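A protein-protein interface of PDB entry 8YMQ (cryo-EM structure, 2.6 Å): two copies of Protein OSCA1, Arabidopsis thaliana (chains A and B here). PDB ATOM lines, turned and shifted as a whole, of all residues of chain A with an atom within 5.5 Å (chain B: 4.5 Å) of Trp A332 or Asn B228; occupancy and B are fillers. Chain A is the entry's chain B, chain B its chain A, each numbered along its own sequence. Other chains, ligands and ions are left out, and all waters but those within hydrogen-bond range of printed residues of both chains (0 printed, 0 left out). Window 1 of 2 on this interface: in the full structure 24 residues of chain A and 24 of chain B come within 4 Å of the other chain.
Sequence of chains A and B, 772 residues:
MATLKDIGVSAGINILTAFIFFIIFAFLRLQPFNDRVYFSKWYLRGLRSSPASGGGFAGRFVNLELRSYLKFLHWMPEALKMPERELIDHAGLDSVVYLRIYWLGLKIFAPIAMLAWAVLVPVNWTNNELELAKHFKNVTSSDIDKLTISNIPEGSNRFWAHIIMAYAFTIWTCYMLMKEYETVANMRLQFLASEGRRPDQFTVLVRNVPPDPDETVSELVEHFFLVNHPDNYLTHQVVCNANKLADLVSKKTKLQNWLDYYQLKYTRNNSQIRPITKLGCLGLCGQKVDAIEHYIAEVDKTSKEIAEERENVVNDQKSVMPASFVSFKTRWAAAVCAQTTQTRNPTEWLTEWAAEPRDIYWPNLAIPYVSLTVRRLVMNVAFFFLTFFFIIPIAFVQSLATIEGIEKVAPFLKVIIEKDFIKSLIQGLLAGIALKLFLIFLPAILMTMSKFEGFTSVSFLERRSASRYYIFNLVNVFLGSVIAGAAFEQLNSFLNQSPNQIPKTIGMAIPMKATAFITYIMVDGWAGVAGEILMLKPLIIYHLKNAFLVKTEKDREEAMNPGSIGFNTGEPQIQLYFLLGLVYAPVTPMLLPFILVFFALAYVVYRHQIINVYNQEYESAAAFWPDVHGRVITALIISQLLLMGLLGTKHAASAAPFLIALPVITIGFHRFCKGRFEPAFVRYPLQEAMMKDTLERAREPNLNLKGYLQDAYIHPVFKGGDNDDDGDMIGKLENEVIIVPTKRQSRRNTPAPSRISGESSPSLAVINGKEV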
ATOM      1  N   ASN A 232      26.861   8.493  31.001  1.00  0.00           N
ATOM      2  CA  ASN A 232      28.121   9.099  30.650  1.00  0.00           C
ATOM      3  C   ASN A 232      28.813   9.933  31.687  1.00  0.00           C
ATOM      4  O   ASN A 232      29.834  10.500  31.400  1.00  0.00           O
ATOM      5  CB  ASN A 232      27.931   9.925  29.396  1.00  0.00           C
ATOM      6  CG  ASN A 232      27.975   9.095  28.134  1.00  0.00           C
ATOM      7  OD1 ASN A 232      28.997   8.498  27.804  1.00  0.00           O
ATOM      8  ND2 ASN A 232      26.862   9.058  27.416  1.00  0.00           N
ATOM      9  N   THR A 330      32.379  10.986  27.485  1.00  0.00           N
ATOM     10  CA  THR A 330      32.509  11.424  26.122  1.00  0.00           C
ATOM     11  C   THR A 330      32.437  12.932  26.023  1.00  0.00           C
ATOM     12  O   THR A 330      32.046  13.595  26.966  1.00  0.00           O
ATOM     13  CB  THR A 330      31.402  10.803  25.272  1.00  0.00           C
ATOM     14  OG1 THR A 330      30.170  10.838  25.989  1.00  0.00           O
ATOM     15  CG2 THR A 330      31.727   9.369  24.940  1.00  0.00           C
ATOM     16  N   ARG A 331      32.834  13.483  24.888  1.00  0.00           N
ATOM     17  CA  ARG A 331      32.742  14.914  24.662  1.00  0.00           C
ATOM     18  C   ARG A 331      31.340  15.216  24.228  1.00  0.00           C
ATOM     19  O   ARG A 331      30.874  16.327  24.387  1.00  0.00           O
ATOM     20  CB  ARG A 331      33.696  15.316  23.556  1.00  0.00           C
ATOM     21  CG  ARG A 331      35.152  15.237  23.928  1.00  0.00           C
ATOM     22  CD  ARG A 331      36.023  15.537  22.737  1.00  0.00           C
ATOM     23  NE  ARG A 331      36.551  14.308  22.179  1.00  0.00           N
ATOM     24  CZ  ARG A 331      37.812  13.923  22.289  1.00  0.00           C
ATOM     25  NH1 ARG A 331      38.692  14.670  22.931  1.00  0.00           N
ATOM     26  NH2 ARG A 331      38.191  12.789  21.745  1.00  0.00           N
ATOM     27  N   TRP A 332      30.655  14.226  23.685  1.00  0.00           N
ATOM     28  CA  TRP A 332      29.281  14.374  23.272  1.00  0.00           C
ATOM     29  C   TRP A 332      28.413  14.599  24.484  1.00  0.00           C
ATOM     30  O   TRP A 332      27.537  15.443  24.459  1.00  0.00           O
ATOM     31  CB  TRP A 332      28.880  13.097  22.533  1.00  0.00           C
ATOM     32  CG  TRP A 332      27.507  13.047  21.965  1.00  0.00           C
ATOM     33  CD1 TRP A 332      27.145  13.354  20.698  1.00  0.00           C
ATOM     34  CD2 TRP A 332      26.314  12.616  22.629  1.00  0.00           C
ATOM     35  NE1 TRP A 332      25.800  13.165  20.528  1.00  0.00           N
ATOM     36  CE2 TRP A 332      25.266  12.718  21.704  1.00  0.00           C
ATOM     37  CE3 TRP A 332      26.031  12.165  23.922  1.00  0.00           C
ATOM     38  CZ2 TRP A 332      23.957  12.388  22.027  1.00  0.00           C
ATOM     39  CZ3 TRP A 332      24.736  11.847  24.241  1.00  0.00           C
ATOM     40  CH2 TRP A 332      23.714  11.955  23.299  1.00  0.00           C
ATOM     41  N   ALA A 333      28.649  13.856  25.553  1.00  0.00           N
ATOM     42  CA  ALA A 333      27.881  13.993  26.777  1.00  0.00           C
ATOM     43  C   ALA A 333      28.108  15.291  27.470  1.00  0.00           C
ATOM     44  O   ALA A 333      27.203  15.836  28.082  1.00  0.00           O
ATOM     45  CB  ALA A 333      28.254  12.896  27.704  1.00  0.00           C
ATOM     46  N   ALA A 334      29.325  15.791  27.400  1.00  0.00           N
ATOM     47  CA  ALA A 334      29.635  17.053  28.001  1.00  0.00           C
ATOM     48  C   ALA A 334      28.992  18.161  27.224  1.00  0.00           C
ATOM     49  O   ALA A 334      28.568  19.138  27.801  1.00  0.00           O
ATOM     50  CB  ALA A 334      31.110  17.225  28.037  1.00  0.00           C
ATOM     51  N   ALA A 335      28.901  18.018  25.912  1.00  0.00           N
ATOM     52  CA  ALA A 335      28.233  19.008  25.100  1.00  0.00           C
ATOM     53  C   ALA A 335      26.768  18.996  25.411  1.00  0.00           C
ATOM     54  O   ALA A 335      26.179  20.041  25.552  1.00  0.00           O
ATOM     55  CB  ALA A 335      28.483  18.744  23.634  1.00  0.00           C
ATOM     56  N   VAL A 336      26.175  17.822  25.546  1.00  0.00           N
ATOM     57  CA  VAL A 336      24.783  17.721  25.928  1.00  0.00           C
ATOM     58  C   VAL A 336      24.550  18.450  27.243  1.00  0.00           C
ATOM     59  O   VAL A 336      23.691  19.299  27.321  1.00  0.00           O
ATOM     60  CB  VAL A 336      24.327  16.249  25.988  1.00  0.00           C
ATOM     61  CG1 VAL A 336      23.039  16.090  26.778  1.00  0.00           C
ATOM     62  CG2 VAL A 336      24.156  15.699  24.588  1.00  0.00           C
ATOM     63  N   CYS A 337      25.354  18.179  28.259  1.00  0.00           N
ATOM     64  CA  CYS A 337      25.208  18.860  29.530  1.00  0.00           C
ATOM     65  C   CYS A 337      25.366  20.366  29.426  1.00  0.00           C
ATOM     66  O   CYS A 337      24.604  21.111  30.018  1.00  0.00           O
ATOM     67  CB  CYS A 337      26.186  18.302  30.539  1.00  0.00           C
ATOM     68  SG  CYS A 337      25.761  18.633  32.249  1.00  0.00           S
ATOM     69  N   LEU A 686      26.919  18.410  18.070  1.00  0.00           N
ATOM     70  CA  LEU A 686      27.001  17.062  18.609  1.00  0.00           C
ATOM     71  C   LEU A 686      27.584  16.063  17.634  1.00  0.00           C
ATOM     72  O   LEU A 686      28.096  15.037  18.044  1.00  0.00           O
ATOM     73  CB  LEU A 686      25.609  16.622  19.053  1.00  0.00           C
ATOM     74  CG  LEU A 686      25.244  16.597  20.538  1.00  0.00           C
ATOM     75  CD1 LEU A 686      25.719  17.824  21.289  1.00  0.00           C
ATOM     76  CD2 LEU A 686      23.746  16.420  20.688  1.00  0.00           C
ATOM     77  N   GLN A 687      27.524  16.357  16.345  1.00  0.00           N
ATOM     78  CA  GLN A 687      28.099  15.485  15.337  1.00  0.00           C
ATOM     79  C   GLN A 687      29.590  15.646  15.361  1.00  0.00           C
ATOM     80  O   GLN A 687      30.321  14.692  15.172  1.00  0.00           O
ATOM     81  CB  GLN A 687      27.547  15.860  13.976  1.00  0.00           C
ATOM     82  CG  GLN A 687      27.982  14.969  12.832  1.00  0.00           C
ATOM     83  CD  GLN A 687      27.991  15.709  11.518  1.00  0.00           C
ATOM     84  OE1 GLN A 687      27.541  15.191  10.501  1.00  0.00           O
ATOM     85  NE2 GLN A 687      28.499  16.934  11.533  1.00  0.00           N
ATOM     86  N   GLU A 688      30.051  16.847  15.644  1.00  0.00           N
ATOM     87  CA  GLU A 688      31.464  17.112  15.714  1.00  0.00           C
ATOM     88  C   GLU A 688      32.040  16.446  16.922  1.00  0.00           C
ATOM     89  O   GLU A 688      33.132  15.899  16.865  1.00  0.00           O
ATOM     90  CB  GLU A 688      31.667  18.617  15.797  1.00  0.00           C
ATOM     91  CG  GLU A 688      32.232  19.258  14.543  1.00  0.00           C
ATOM     92  CD  GLU A 688      31.388  19.007  13.308  1.00  0.00           C
ATOM     93  OE1 GLU A 688      31.965  18.638  12.267  1.00  0.00           O
ATOM     94  OE2 GLU A 688      30.155  19.180  13.368  1.00  0.00           O
ATOM     95  N   ALA A 689      31.306  16.473  18.020  1.00  0.00           N
ATOM     96  CA  ALA A 689      31.751  15.850  19.250  1.00  0.00           C
ATOM     97  C   ALA A 689      31.837  14.365  19.096  1.00  0.00           C
ATOM     98  O   ALA A 689      32.811  13.767  19.507  1.00  0.00           O
ATOM     99  CB  ALA A 689      30.791  16.196  20.354  1.00  0.00           C
ATOM    100  N   MET A 690      30.826  13.762  18.489  1.00  0.00           N
ATOM    101  CA  MET A 690      30.831  12.339  18.262  1.00  0.00           C
ATOM    102  C   MET A 690      31.954  11.909  17.345  1.00  0.00           C
ATOM    103  O   MET A 690      32.588  10.907  17.595  1.00  0.00           O
ATOM    104  CB  MET A 690      29.492  11.875  17.714  1.00  0.00           C
ATOM    105  CG  MET A 690      29.300  10.369  17.726  1.00  0.00           C
ATOM    106  SD  MET A 690      28.449   9.774  19.193  1.00  0.00           S
ATOM    107  CE  MET A 690      29.826   9.272  20.220  1.00  0.00           C
ATOM    108  N   ASP A 693      35.164  11.885  19.368  1.00  0.00           N
ATOM    109  CA  ASP A 693      35.140  10.761  20.283  1.00  0.00           C
ATOM    110  C   ASP A 693      35.417   9.446  19.609  1.00  0.00           C
ATOM    111  O   ASP A 693      36.215   8.671  20.100  1.00  0.00           O
ATOM    112  CB  ASP A 693      33.771  10.683  20.935  1.00  0.00           C
ATOM    113  CG  ASP A 693      33.601  11.661  22.049  1.00  0.00           C
ATOM    114  OD1 ASP A 693      34.564  11.876  22.808  1.00  0.00           O
ATOM    115  OD2 ASP A 693      32.492  12.206  22.172  1.00  0.00           O
ATOM    116  N   PHE B 224      21.978   9.368  10.596  1.00  0.00           N
ATOM    117  CA  PHE B 224      22.387  10.456  11.460  1.00  0.00           C
ATOM    118  C   PHE B 224      22.049  10.163  12.882  1.00  0.00           C
ATOM    119  O   PHE B 224      22.868  10.315  13.756  1.00  0.00           O
ATOM    120  CB  PHE B 224      21.676  11.739  11.061  1.00  0.00           C
ATOM    121  CG  PHE B 224      22.203  12.975  11.731  1.00  0.00           C
ATOM    122  CD1 PHE B 224      23.285  13.648  11.205  1.00  0.00           C
ATOM    123  CD2 PHE B 224      21.593  13.483  12.864  1.00  0.00           C
ATOM    124  CE1 PHE B 224      23.766  14.790  11.808  1.00  0.00           C
ATOM    125  CE2 PHE B 224      22.070  14.618  13.474  1.00  0.00           C
ATOM    126  CZ  PHE B 224      23.158  15.272  12.945  1.00  0.00           C
ATOM    127  N   PHE B 225      20.834   9.735  13.134  1.00  0.00           N
ATOM    128  CA  PHE B 225      20.417   9.558  14.504  1.00  0.00           C
ATOM    129  C   PHE B 225      20.843   8.251  15.107  1.00  0.00           C
ATOM    130  O   PHE B 225      20.640   8.030  16.269  1.00  0.00           O
ATOM    131  CB  PHE B 225      18.920   9.804  14.621  1.00  0.00           C
ATOM    132  CG  PHE B 225      18.542  11.243  14.454  1.00  0.00           C
ATOM    133  CD1 PHE B 225      18.616  12.111  15.517  1.00  0.00           C
ATOM    134  CD2 PHE B 225      18.135  11.729  13.228  1.00  0.00           C
ATOM    135  CE1 PHE B 225      18.282  13.437  15.365  1.00  0.00           C
ATOM    136  CE2 PHE B 225      17.803  13.053  13.066  1.00  0.00           C
ATOM    137  CZ  PHE B 225      17.873  13.910  14.139  1.00  0.00           C
ATOM    138  N   LEU B 226      21.462   7.387  14.334  1.00  0.00           N
ATOM    139  CA  LEU B 226      21.976   6.157  14.884  1.00  0.00           C
ATOM    140  C   LEU B 226      23.442   6.337  15.188  1.00  0.00           C
ATOM    141  O   LEU B 226      24.030   5.528  15.885  1.00  0.00           O
ATOM    142  CB  LEU B 226      21.775   5.010  13.906  1.00  0.00           C
ATOM    143  CG  LEU B 226      21.210   3.692  14.422  1.00  0.00           C
ATOM    144  CD1 LEU B 226      20.721   3.808  15.856  1.00  0.00           C
ATOM    145  CD2 LEU B 226      20.108   3.205  13.502  1.00  0.00           C
ATOM    146  N   VAL B 227      24.049   7.386  14.655  1.00  0.00           N
ATOM    147  CA  VAL B 227      25.442   7.666  14.952  1.00  0.00           C
ATOM    148  C   VAL B 227      25.596   8.817  15.911  1.00  0.00           C
ATOM    149  O   VAL B 227      26.557   8.856  16.653  1.00  0.00           O
ATOM    150  CB  VAL B 227      26.327   7.866  13.686  1.00  0.00           C
ATOM    151  CG1 VAL B 227      26.227   6.672  12.756  1.00  0.00           C
ATOM    152  CG2 VAL B 227      26.051   9.162  12.956  1.00  0.00           C
ATOM    153  N   ASN B 228      24.647   9.737  15.935  1.00  0.00           N
ATOM    154  CA  ASN B 228      24.786  10.921  16.762  1.00  0.00           C
ATOM    155  C   ASN B 228      23.938  10.851  17.992  1.00  0.00           C
ATOM    156  O   ASN B 228      24.218  11.543  18.958  1.00  0.00           O
ATOM    157  CB  ASN B 228      24.516  12.174  15.949  1.00  0.00           C
ATOM    158  CG  ASN B 228      25.549  12.389  14.875  1.00  0.00           C
ATOM    159  OD1 ASN B 228      25.238  12.409  13.694  1.00  0.00           O
ATOM    160  ND2 ASN B 228      26.798  12.527  15.284  1.00  0.00           N
ATOM    161  N   HIS B 229      22.900  10.033  17.980  1.00  0.00           N
ATOM    162  CA  HIS B 229      22.099   9.812  19.171  1.00  0.00           C
ATOM    163  C   HIS B 229      21.985   8.320  19.193  1.00  0.00           C
ATOM    164  O   HIS B 229      20.891   7.788  19.140  1.00  0.00           O
ATOM    165  CB  HIS B 229      20.736  10.453  19.027  1.00  0.00           C
ATOM    166  CG  HIS B 229      20.763  11.945  19.104  1.00  0.00           C
ATOM    167  ND1 HIS B 229      20.624  12.631  20.290  1.00  0.00           N
ATOM    168  CD2 HIS B 229      20.924  12.885  18.144  1.00  0.00           C
ATOM    169  CE1 HIS B 229      20.696  13.928  20.057  1.00  0.00           C
ATOM    170  NE2 HIS B 229      20.876  14.108  18.763  1.00  0.00           N
ATOM    171  N   PRO B 230      23.113   7.622  19.350  1.00  0.00           N
ATOM    172  CA  PRO B 230      23.096   6.169  19.206  1.00  0.00           C
ATOM    173  C   PRO B 230      22.259   5.353  20.156  1.00  0.00           C
ATOM    174  O   PRO B 230      21.554   4.458  19.705  1.00  0.00           O
ATOM    175  CB  PRO B 230      24.567   5.799  19.409  1.00  0.00           C
ATOM    176  CG  PRO B 230      25.324   7.070  19.601  1.00  0.00           C
ATOM    177  CD  PRO B 230      24.318   8.056  20.070  1.00  0.00           C
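SD of Met A690 sits close to O of Val B227, at 3.3 Å.
O of Asn B228 sits at hydrogen-bond distance from NE1 of Trp A332 (2.8 Å).
The backbone carbonyl oxygen of Phe B224 lies close to the side-chain amide oxygen of Asn B228 (3.2 Å).
The side-chain amide nitrogen (NE2) of Gln A687 lies within hydrogen-bond range of the side-chain carboxylate (OE2) of Glu A688, 3.3 Å away.
The backbone NH (N) of Trp A332 lies within hydrogen-bond range of the side-chain carboxylate (OD2) of Asp A693 (3.1 Å).
Among the printed residues, merely in contact across the chains: Gln A687 with Asn B228, Met A690 with Asn B228, Trp A332 with His B229, Leu A686 with Asn B228 and Leu A686 with His B229.
Trp A332 touches just these residues of chain B: Asn B228 and His B229.
Cys A337 touches none of the printed residues of chain B.
Printed residues of chain B within 4 Å of Leu A686: Asn B228 and His B229.
Ala A689 touches none of the printed residues of chain B.
Printed residues of chain A within 4 Å of Val B227: Met A690 (3.3 Å).
Asn B228 touches just these residues of chain A: Trp A332, Leu A686, Gln A687 and Met A690.
Of the printed residues of chain A, His B229 touches Trp A332 (3.8 Å) and Leu A686 (3.99 Å).
The nearest printed residue of chain B that does not touch Trp A332 is Pro B230 (4.8 Å).
Of the 7 printed residues of chain B, 3 touch a printed residue of chain A.
Hydrophobic or aromatic side chains of chain B within 4 Å of the printed part of chain A: His B229.
Of the 15 printed residues of chain A, 4 touch a printed residue of chain B.
Hydrophobic or aromatic side chains of chain A within 4 Å of the printed part of chain B: Trp A332, Leu A686 and Met A690.
Along chain A the printed residues that touch a printed residue of chain B span positions 332 to 690.
No position is printed for both chains.
Of the 7 pairs that touch across the chains among the printed residues, none has its exchanged pair printed and touching as well.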
